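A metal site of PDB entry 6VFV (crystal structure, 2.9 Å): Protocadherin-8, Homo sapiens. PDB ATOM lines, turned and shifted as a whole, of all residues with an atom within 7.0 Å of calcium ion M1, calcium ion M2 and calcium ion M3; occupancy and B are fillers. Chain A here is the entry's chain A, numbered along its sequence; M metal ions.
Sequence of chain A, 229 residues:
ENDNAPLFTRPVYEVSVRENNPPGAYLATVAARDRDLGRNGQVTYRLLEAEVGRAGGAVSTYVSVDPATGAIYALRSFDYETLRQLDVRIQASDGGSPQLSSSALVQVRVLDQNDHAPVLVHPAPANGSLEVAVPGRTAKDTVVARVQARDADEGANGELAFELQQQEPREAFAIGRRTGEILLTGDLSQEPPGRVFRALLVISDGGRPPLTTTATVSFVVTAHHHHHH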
ATOM      1  N   GLU A  19      12.223  -2.765  13.301  1.00  0.00           N
ATOM      2  CA  GLU A  19      12.295  -1.801  12.210  1.00  0.00           C
ATOM      3  C   GLU A  19      13.654  -1.113  12.165  1.00  0.00           C
ATOM      4  O   GLU A  19      14.368  -1.011  13.171  1.00  0.00           O
ATOM      5  CB  GLU A  19      11.170  -0.774  12.391  1.00  0.00           C
ATOM      6  CG  GLU A  19      11.047   0.273  11.318  1.00  0.00           C
ATOM      7  CD  GLU A  19      10.023   1.333  11.691  1.00  0.00           C
ATOM      8  OE1 GLU A  19       9.484   1.266  12.819  1.00  0.00           O
ATOM      9  OE2 GLU A  19       9.760   2.222  10.855  1.00  0.00           O
ATOM     10  N   ASN A  20      14.017  -0.633  10.977  1.00  0.00           N
ATOM     11  CA  ASN A  20      15.246   0.137  10.759  1.00  0.00           C
ATOM     12  C   ASN A  20      16.488  -0.692  11.102  1.00  0.00           C
ATOM     13  O   ASN A  20      17.418  -0.219  11.769  1.00  0.00           O
ATOM     14  CB  ASN A  20      15.223   1.443  11.556  1.00  0.00           C
ATOM     15  CG  ASN A  20      13.962   2.264  11.297  1.00  0.00           C
ATOM     16  OD1 ASN A  20      13.550   2.454  10.148  1.00  0.00           O
ATOM     17  ND2 ASN A  20      13.341   2.737  12.363  1.00  0.00           N
ATOM     18  N   PHE A  78      14.180  -2.499   7.253  1.00  0.00           N
ATOM     19  CA  PHE A  78      12.735  -2.664   7.172  1.00  0.00           C
ATOM     20  C   PHE A  78      12.032  -1.498   7.866  1.00  0.00           C
ATOM     21  O   PHE A  78      12.454  -1.052   8.931  1.00  0.00           O
ATOM     22  CB  PHE A  78      12.306  -3.988   7.807  1.00  0.00           C
ATOM     23  CG  PHE A  78      12.923  -5.198   7.159  1.00  0.00           C
ATOM     24  CD1 PHE A  78      13.408  -6.243   7.922  1.00  0.00           C
ATOM     25  CD2 PHE A  78      13.000  -5.296   5.770  1.00  0.00           C
ATOM     26  CE1 PHE A  78      13.970  -7.358   7.318  1.00  0.00           C
ATOM     27  CE2 PHE A  78      13.556  -6.405   5.173  1.00  0.00           C
ATOM     28  CZ  PHE A  78      14.044  -7.439   5.943  1.00  0.00           C
ATOM     29  N   ASP A  79      10.958  -1.030   7.241  1.00  0.00           N
ATOM     30  CA  ASP A  79      10.132   0.061   7.761  1.00  0.00           C
ATOM     31  C   ASP A  79       8.767  -0.502   8.156  1.00  0.00           C
ATOM     32  O   ASP A  79       8.018  -0.977   7.298  1.00  0.00           O
ATOM     33  CB  ASP A  79       9.981   1.170   6.721  1.00  0.00           C
ATOM     34  CG  ASP A  79       9.035   2.262   7.176  1.00  0.00           C
ATOM     35  OD1 ASP A  79       8.810   2.383   8.396  1.00  0.00           O
ATOM     36  OD2 ASP A  79       8.541   3.013   6.301  1.00  0.00           O
ATOM     37  N   TYR A  80       8.462  -0.455   9.451  1.00  0.00           N
ATOM     38  CA  TYR A  80       7.223  -1.064   9.940  1.00  0.00           C
ATOM     39  C   TYR A  80       6.004  -0.355   9.363  1.00  0.00           C
ATOM     40  O   TYR A  80       4.996  -1.001   9.040  1.00  0.00           O
ATOM     41  CB  TYR A  80       7.193  -1.034  11.469  1.00  0.00           C
ATOM     42  CG  TYR A  80       5.900  -1.561  12.059  1.00  0.00           C
ATOM     43  CD1 TYR A  80       5.720  -2.917  12.276  1.00  0.00           C
ATOM     44  CD2 TYR A  80       4.862  -0.703  12.392  1.00  0.00           C
ATOM     45  CE1 TYR A  80       4.548  -3.408  12.811  1.00  0.00           C
ATOM     46  CE2 TYR A  80       3.678  -1.178  12.918  1.00  0.00           C
ATOM     47  CZ  TYR A  80       3.524  -2.533  13.125  1.00  0.00           C
ATOM     48  OH  TYR A  80       2.343  -2.996  13.659  1.00  0.00           O
ATOM     49  N   GLU A  81       6.060   0.967   9.230  1.00  0.00           N
ATOM     50  CA  GLU A  81       4.939   1.698   8.652  1.00  0.00           C
ATOM     51  C   GLU A  81       4.708   1.321   7.192  1.00  0.00           C
ATOM     52  O   GLU A  81       3.637   1.574   6.657  1.00  0.00           O
ATOM     53  CB  GLU A  81       5.171   3.205   8.778  1.00  0.00           C
ATOM     54  CG  GLU A  81       4.991   3.755  10.195  1.00  0.00           C
ATOM     55  CD  GLU A  81       6.112   3.350  11.140  1.00  0.00           C
ATOM     56  OE1 GLU A  81       7.288   3.632  10.832  1.00  0.00           O
ATOM     57  OE2 GLU A  81       5.811   2.735  12.185  1.00  0.00           O
ATOM     58  N   THR A  82       5.702   0.706   6.542  1.00  0.00           N
ATOM     59  CA  THR A  82       5.614   0.300   5.143  1.00  0.00           C
ATOM     60  C   THR A  82       5.388  -1.189   4.960  1.00  0.00           C
ATOM     61  O   THR A  82       4.862  -1.589   3.911  1.00  0.00           O
ATOM     62  CB  THR A  82       6.908   0.717   4.416  1.00  0.00           C
ATOM     63  OG1 THR A  82       6.948   2.142   4.274  1.00  0.00           O
ATOM     64  CG2 THR A  82       7.022   0.066   3.033  1.00  0.00           C
ATOM     65  N   LEU A 111       8.906  -5.709  13.865  1.00  0.00           N
ATOM     66  CA  LEU A 111       8.455  -5.037  15.070  1.00  0.00           C
ATOM     67  C   LEU A 111       8.647  -3.531  14.935  1.00  0.00           C
ATOM     68  O   LEU A 111       9.506  -3.059  14.181  1.00  0.00           O
ATOM     69  CB  LEU A 111       9.214  -5.536  16.295  1.00  0.00           C
ATOM     70  CG  LEU A 111       9.281  -7.042  16.500  1.00  0.00           C
ATOM     71  CD1 LEU A 111      10.481  -7.384  17.349  1.00  0.00           C
ATOM     72  CD2 LEU A 111       8.007  -7.550  17.135  1.00  0.00           C
ATOM     73  N   ASP A 112       7.849  -2.792  15.682  1.00  0.00           N
ATOM     74  CA  ASP A 112       7.859  -1.340  15.601  1.00  0.00           C
ATOM     75  C   ASP A 112       8.988  -0.761  16.445  1.00  0.00           C
ATOM     76  O   ASP A 112       9.391  -1.309  17.474  1.00  0.00           O
ATOM     77  CB  ASP A 112       6.517  -0.770  16.055  1.00  0.00           C
ATOM     78  CG  ASP A 112       6.452   0.736  15.930  1.00  0.00           C
ATOM     79  OD1 ASP A 112       7.113   1.293  15.023  1.00  0.00           O
ATOM     80  OD2 ASP A 112       5.738   1.375  16.737  1.00  0.00           O
ATOM     81  N   GLN A 113       9.512   0.364  15.977  1.00  0.00           N
ATOM     82  CA  GLN A 113      10.506   1.175  16.671  1.00  0.00           C
ATOM     83  C   GLN A 113       9.936   2.581  16.793  1.00  0.00           C
ATOM     84  O   GLN A 113       9.216   3.050  15.914  1.00  0.00           O
ATOM     85  CB  GLN A 113      11.831   1.172  15.893  1.00  0.00           C
ATOM     86  CG  GLN A 113      13.034   1.837  16.555  1.00  0.00           C
ATOM     87  CD  GLN A 113      14.292   1.756  15.683  1.00  0.00           C
ATOM     88  OE1 GLN A 113      14.282   1.103  14.647  1.00  0.00           O
ATOM     89  NE2 GLN A 113      15.351   2.415  16.112  1.00  0.00           N
ATOM     90  N   ASN A 114      10.222   3.258  17.907  1.00  0.00           N
ATOM     91  CA  ASN A 114       9.737   4.627  18.082  1.00  0.00           C
ATOM     92  C   ASN A 114      10.649   5.548  17.270  1.00  0.00           C
ATOM     93  O   ASN A 114      11.595   6.161  17.770  1.00  0.00           O
ATOM     94  CB  ASN A 114       9.691   5.033  19.543  1.00  0.00           C
ATOM     95  CG  ASN A 114       8.837   6.275  19.776  1.00  0.00           C
ATOM     96  OD1 ASN A 114       8.088   6.684  18.893  1.00  0.00           O
ATOM     97  ND2 ASN A 114       8.946   6.874  20.952  1.00  0.00           N
ATOM     98  N   ASP A 115      10.340   5.634  15.969  1.00  0.00           N
ATOM     99  CA  ASP A 115      11.118   6.421  15.023  1.00  0.00           C
ATOM    100  C   ASP A 115      10.281   7.570  14.459  1.00  0.00           C
ATOM    101  O   ASP A 115      10.499   8.015  13.323  1.00  0.00           O
ATOM    102  CB  ASP A 115      11.666   5.546  13.900  1.00  0.00           C
ATOM    103  CG  ASP A 115      10.581   4.830  13.145  1.00  0.00           C
ATOM    104  OD1 ASP A 115       9.506   4.579  13.738  1.00  0.00           O
ATOM    105  OD2 ASP A 115      10.791   4.511  11.956  1.00  0.00           O
ATOM    106  N   HIS A 116       9.312   8.052  15.224  1.00  0.00           N
ATOM    107  CA  HIS A 116       8.508   9.208  14.849  1.00  0.00           C
ATOM    108  C   HIS A 116       8.260  10.056  16.082  1.00  0.00           C
ATOM    109  O   HIS A 116       7.692   9.578  17.073  1.00  0.00           O
ATOM    110  CB  HIS A 116       7.176   8.803  14.202  1.00  0.00           C
ATOM    111  CG  HIS A 116       7.306   8.384  12.773  1.00  0.00           C
ATOM    112  ND1 HIS A 116       7.126   7.089  12.357  1.00  0.00           N
ATOM    113  CD2 HIS A 116       7.581   9.109  11.663  1.00  0.00           C
ATOM    114  CE1 HIS A 116       7.287   7.018  11.043  1.00  0.00           C
ATOM    115  NE2 HIS A 116       7.556   8.236  10.601  1.00  0.00           N
ATOM    116  N   ALA A 117       8.672  11.266  16.036  1.00  0.00           N
ATOM    117  CA  ALA A 117       8.261  12.194  17.071  1.00  0.00           C
ATOM    118  C   ALA A 117       6.912  12.804  16.705  1.00  0.00           C
ATOM    119  O   ALA A 117       6.589  12.935  15.524  1.00  0.00           O
ATOM    120  CB  ALA A 117       9.302  13.299  17.232  1.00  0.00           C
ATOM    121  N   PRO A 118       6.093  13.170  17.687  1.00  0.00           N
ATOM    122  CA  PRO A 118       4.812  13.801  17.359  1.00  0.00           C
ATOM    123  C   PRO A 118       5.026  15.047  16.510  1.00  0.00           C
ATOM    124  O   PRO A 118       5.983  15.784  16.685  1.00  0.00           O
ATOM    125  CB  PRO A 118       4.208  14.134  18.725  1.00  0.00           C
ATOM    126  CG  PRO A 118       5.347  14.043  19.698  1.00  0.00           C
ATOM    127  CD  PRO A 118       6.290  13.038  19.137  1.00  0.00           C
ATOM    128  N   ASP A 151       1.114  11.080  15.345  1.00  0.00           N
ATOM    129  CA  ASP A 151       2.278  10.231  15.535  1.00  0.00           C
ATOM    130  C   ASP A 151       2.017   8.912  14.829  1.00  0.00           C
ATOM    131  O   ASP A 151       0.993   8.267  15.075  1.00  0.00           O
ATOM    132  CB  ASP A 151       2.557  10.004  17.022  1.00  0.00           C
ATOM    133  CG  ASP A 151       3.920   9.361  17.290  1.00  0.00           C
ATOM    134  OD1 ASP A 151       4.313   8.442  16.524  1.00  0.00           O
ATOM    135  OD2 ASP A 151       4.593   9.768  18.252  1.00  0.00           O
ATOM    136  N   ALA A 152       2.931   8.520  13.958  1.00  0.00           N
ATOM    137  CA  ALA A 152       2.713   7.371  13.082  1.00  0.00           C
ATOM    138  C   ALA A 152       2.976   6.038  13.756  1.00  0.00           C
ATOM    139  O   ALA A 152       2.572   5.005  13.200  1.00  0.00           O
ATOM    140  CB  ALA A 152       3.605   7.495  11.851  1.00  0.00           C
ATOM    141  N   ASP A 153       3.622   6.021  14.916  1.00  0.00           N
ATOM    142  CA  ASP A 153       4.071   4.772  15.515  1.00  0.00           C
ATOM    143  C   ASP A 153       2.887   4.008  16.116  1.00  0.00           C
ATOM    144  O   ASP A 153       1.727   4.400  15.993  1.00  0.00           O
ATOM    145  CB  ASP A 153       5.156   5.065  16.549  1.00  0.00           C
ATOM    146  CG  ASP A 153       6.397   5.693  15.939  1.00  0.00           C
ATOM    147  OD1 ASP A 153       6.816   5.257  14.833  1.00  0.00           O
ATOM    148  OD2 ASP A 153       6.963   6.623  16.558  1.00  0.00           O
ATOM    149  N   GLU A 154       3.200   2.892  16.770  1.00  0.00           N
ATOM    150  CA  GLU A 154       2.205   1.952  17.272  1.00  0.00           C
ATOM    151  C   GLU A 154       2.113   2.031  18.787  1.00  0.00           C
ATOM    152  O   GLU A 154       3.021   2.497  19.473  1.00  0.00           O
ATOM    153  CB  GLU A 154       2.566   0.527  16.831  1.00  0.00           C
ATOM    154  CG  GLU A 154       1.721  -0.574  17.451  1.00  0.00           C
ATOM    155  CD  GLU A 154       1.994  -1.939  16.842  1.00  0.00           C
ATOM    156  OE1 GLU A 154       2.975  -2.062  16.090  1.00  0.00           O
ATOM    157  OE2 GLU A 154       1.229  -2.890  17.138  1.00  0.00           O
ATOM    158  N   ALA A 156       1.747   2.708  22.584  1.00  0.00           N
ATOM    159  CA  ALA A 156       2.094   3.910  23.335  1.00  0.00           C
ATOM    160  C   ALA A 156       3.004   4.830  22.536  1.00  0.00           C
ATOM    161  O   ALA A 156       2.997   6.054  22.757  1.00  0.00           O
ATOM    162  CB  ALA A 156       2.767   3.535  24.665  1.00  0.00           C
ATOM    163  N   ASN A 157       3.789   4.289  21.597  1.00  0.00           N
ATOM    164  CA  ASN A 157       4.622   5.136  20.752  1.00  0.00           C
ATOM    165  C   ASN A 157       3.816   6.115  19.911  1.00  0.00           C
ATOM    166  O   ASN A 157       4.399   7.024  19.320  1.00  0.00           O
ATOM    167  CB  ASN A 157       5.497   4.281  19.828  1.00  0.00           C
ATOM    168  CG  ASN A 157       6.556   3.499  20.582  1.00  0.00           C
ATOM    169  OD1 ASN A 157       7.115   3.981  21.573  1.00  0.00           O
ATOM    170  ND2 ASN A 157       6.849   2.296  20.114  1.00  0.00           N
ATOM    171  N   GLY A 158       2.503   5.945  19.833  1.00  0.00           N
ATOM    172  CA  GLY A 158       1.639   6.903  19.163  1.00  0.00           C
ATOM    173  C   GLY A 158       0.650   7.539  20.120  1.00  0.00           C
ATOM    174  O   GLY A 158      -0.188   8.352  19.715  1.00  0.00           O
ATOM    175  N   GLU A 159       0.743   7.177  21.404  1.00  0.00           N
ATOM    176  CA  GLU A 159      -0.143   7.719  22.430  1.00  0.00           C
ATOM    177  C   GLU A 159       0.392   9.076  22.878  1.00  0.00           C
ATOM    178  O   GLU A 159       1.426   9.155  23.547  1.00  0.00           O
ATOM    179  CB  GLU A 159      -0.242   6.742  23.603  1.00  0.00           C
ATOM    180  CG  GLU A 159      -1.308   7.074  24.618  1.00  0.00           C
ATOM    181  CD  GLU A 159      -1.476   5.979  25.667  1.00  0.00           C
ATOM    182  OE1 GLU A 159      -0.625   5.064  25.722  1.00  0.00           O
ATOM    183  OE2 GLU A 159      -2.463   6.044  26.431  1.00  0.00           O
ATOM    184  N   LEU A 160      -0.311  10.150  22.516  1.00  0.00           N
ATOM    185  CA  LEU A 160       0.169  11.506  22.722  1.00  0.00           C
ATOM    186  C   LEU A 160      -0.373  12.115  24.014  1.00  0.00           C
ATOM    187  O   LEU A 160      -1.419  11.727  24.531  1.00  0.00           O
ATOM    188  CB  LEU A 160      -0.214  12.397  21.543  1.00  0.00           C
ATOM    189  CG  LEU A 160       0.442  12.060  20.190  1.00  0.00           C
ATOM    190  CD1 LEU A 160       0.363  13.270  19.260  1.00  0.00           C
ATOM    191  CD2 LEU A 160       1.892  11.600  20.357  1.00  0.00           C
ATOM    192  N   ASP A 205       4.988  11.616  23.401  1.00  0.00           N
ATOM    193  CA  ASP A 205       4.423  10.303  23.106  1.00  0.00           C
ATOM    194  C   ASP A 205       4.810   9.338  24.214  1.00  0.00           C
ATOM    195  O   ASP A 205       5.571   9.674  25.121  1.00  0.00           O
ATOM    196  CB  ASP A 205       4.875   9.806  21.725  1.00  0.00           C
ATOM    197  CG  ASP A 205       6.313   9.313  21.712  1.00  0.00           C
ATOM    198  OD1 ASP A 205       7.041   9.514  22.706  1.00  0.00           O
ATOM    199  OD2 ASP A 205       6.716   8.737  20.680  1.00  0.00           O
ATOM    200  N   GLY A 206       4.265   8.122  24.143  1.00  0.00           N
ATOM    201  CA  GLY A 206       4.403   7.197  25.248  1.00  0.00           C
ATOM    202  C   GLY A 206       5.582   6.253  25.132  1.00  0.00           C
ATOM    203  O   GLY A 206       5.523   5.120  25.609  1.00  0.00           O
ATOM    204  N   GLY A 207       6.658   6.705  24.491  1.00  0.00           N
ATOM    205  CA  GLY A 207       7.846   5.883  24.356  1.00  0.00           C
ATOM    206  C   GLY A 207       8.677   5.839  25.625  1.00  0.00           C
ATOM    207  O   GLY A 207       8.456   6.568  26.596  1.00  0.00           O
ATOM    208  N   LEU A 211       9.582  10.568  22.854  1.00  0.00           N
ATOM    209  CA  LEU A 211       9.965  11.586  21.889  1.00  0.00           C
ATOM    210  C   LEU A 211       9.055  12.796  22.057  1.00  0.00           C
ATOM    211  O   LEU A 211       7.834  12.659  22.055  1.00  0.00           O
ATOM    212  CB  LEU A 211       9.902  11.054  20.462  1.00  0.00           C
ATOM    213  CG  LEU A 211      10.934   9.983  20.091  1.00  0.00           C
ATOM    214  CD1 LEU A 211      11.012   9.822  18.587  1.00  0.00           C
ATOM    215  CD2 LEU A 211      12.323  10.298  20.644  1.00  0.00           C
HETATM  216 CA    CA M   1       6.334   8.166  18.449  1.00  0.00          CA
HETATM  217 CA    CA M   2       7.776   3.157  13.890  1.00  0.00          CA
HETATM  218 CA    CA M   3       9.614   4.031   9.689  1.00  0.00          CA
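Calcium ion M3 is bound by OE2 of Glu 19, OD1 of Asp 79, OD2 of Asp 115 and OE1 of Glu 81.
Calcium ion M1 is bound by OD2 of Asp 205 (2.3 Å), OD1 of Asn 114 (2.3 Å), OD2 of Asp 151 (2.4 Å), O of His 116 (2.4 Å), O of Asn 157 (2.4 Å), OD2 of Asp 153 (2.5 Å) and OD1 of Asp 151 (2.8 Å). Calcium ion M1 has seven donor atoms within binding distance.
Six residues have an atom within 4 Å of calcium ion M1: Asn 114, His 116, Asp 151, Asp 153, Asn 157 and Asp 205. The nearest printed residue that does not touch calcium ion M1 is Ala 117 (4.6 Å).
Within 4 Å of calcium ion M3: Glu 19, Asp 79, Glu 81 and Asp 115.
Calcium ion M2 is bound by the side-chain carboxylate of Asp 115 (2.2 Å), the side-chain carboxylate of Asp 112 (2.3 Å), the backbone carbonyl oxygen of Gln 113 (2.5 Å), the side-chain carboxylate of Asp 153 (2.5 Å), the side-chain carboxylate of Glu 81 (2.6 Å) and the side-chain carboxylate of Glu 19 (2.8 Å). Slightly farther from calcium ion M2 lies OE1 of Glu 81 (3.1 Å).
The side-chain carboxylate of Asp 79 is in hydrogen-bond range of the side-chain hydroxyl of Thr 82 (2.7 Å). OD1 of Asp 205 lies within hydrogen-bond range of N of Leu 211 (2.8 Å). The side-chain carboxylate (OD1) of Asp 205 lies close to the backbone NH (N) of Gly 207, at 3.4 Å. OE1 of Gln 113 is in hydrogen-bond range of ND2 of Asn 20 (3.0 Å). N of Glu 19 lies within hydrogen-bond range of O of Leu 111, 2.9 Å away. The side-chain carboxylate (OE2) of Glu 19 sits close to the backbone NH (N) of Tyr 80, at 3.3 Å. OD2 of Asp 115 sits close to ND2 of Asn 20 (3.1 Å). The side-chain carboxylate (OD2) of Asp 112 is in hydrogen-bond range of the backbone NH (N) of Glu 154, at 3.0 Å.
Six residues have an atom within 4 Å of calcium ion M2: Glu 19, Glu 81, Asp 112, Gln 113, Asp 115 and Asp 153. The nearest printed residue that does not touch calcium ion M2 is His 116 (4.3 Å).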
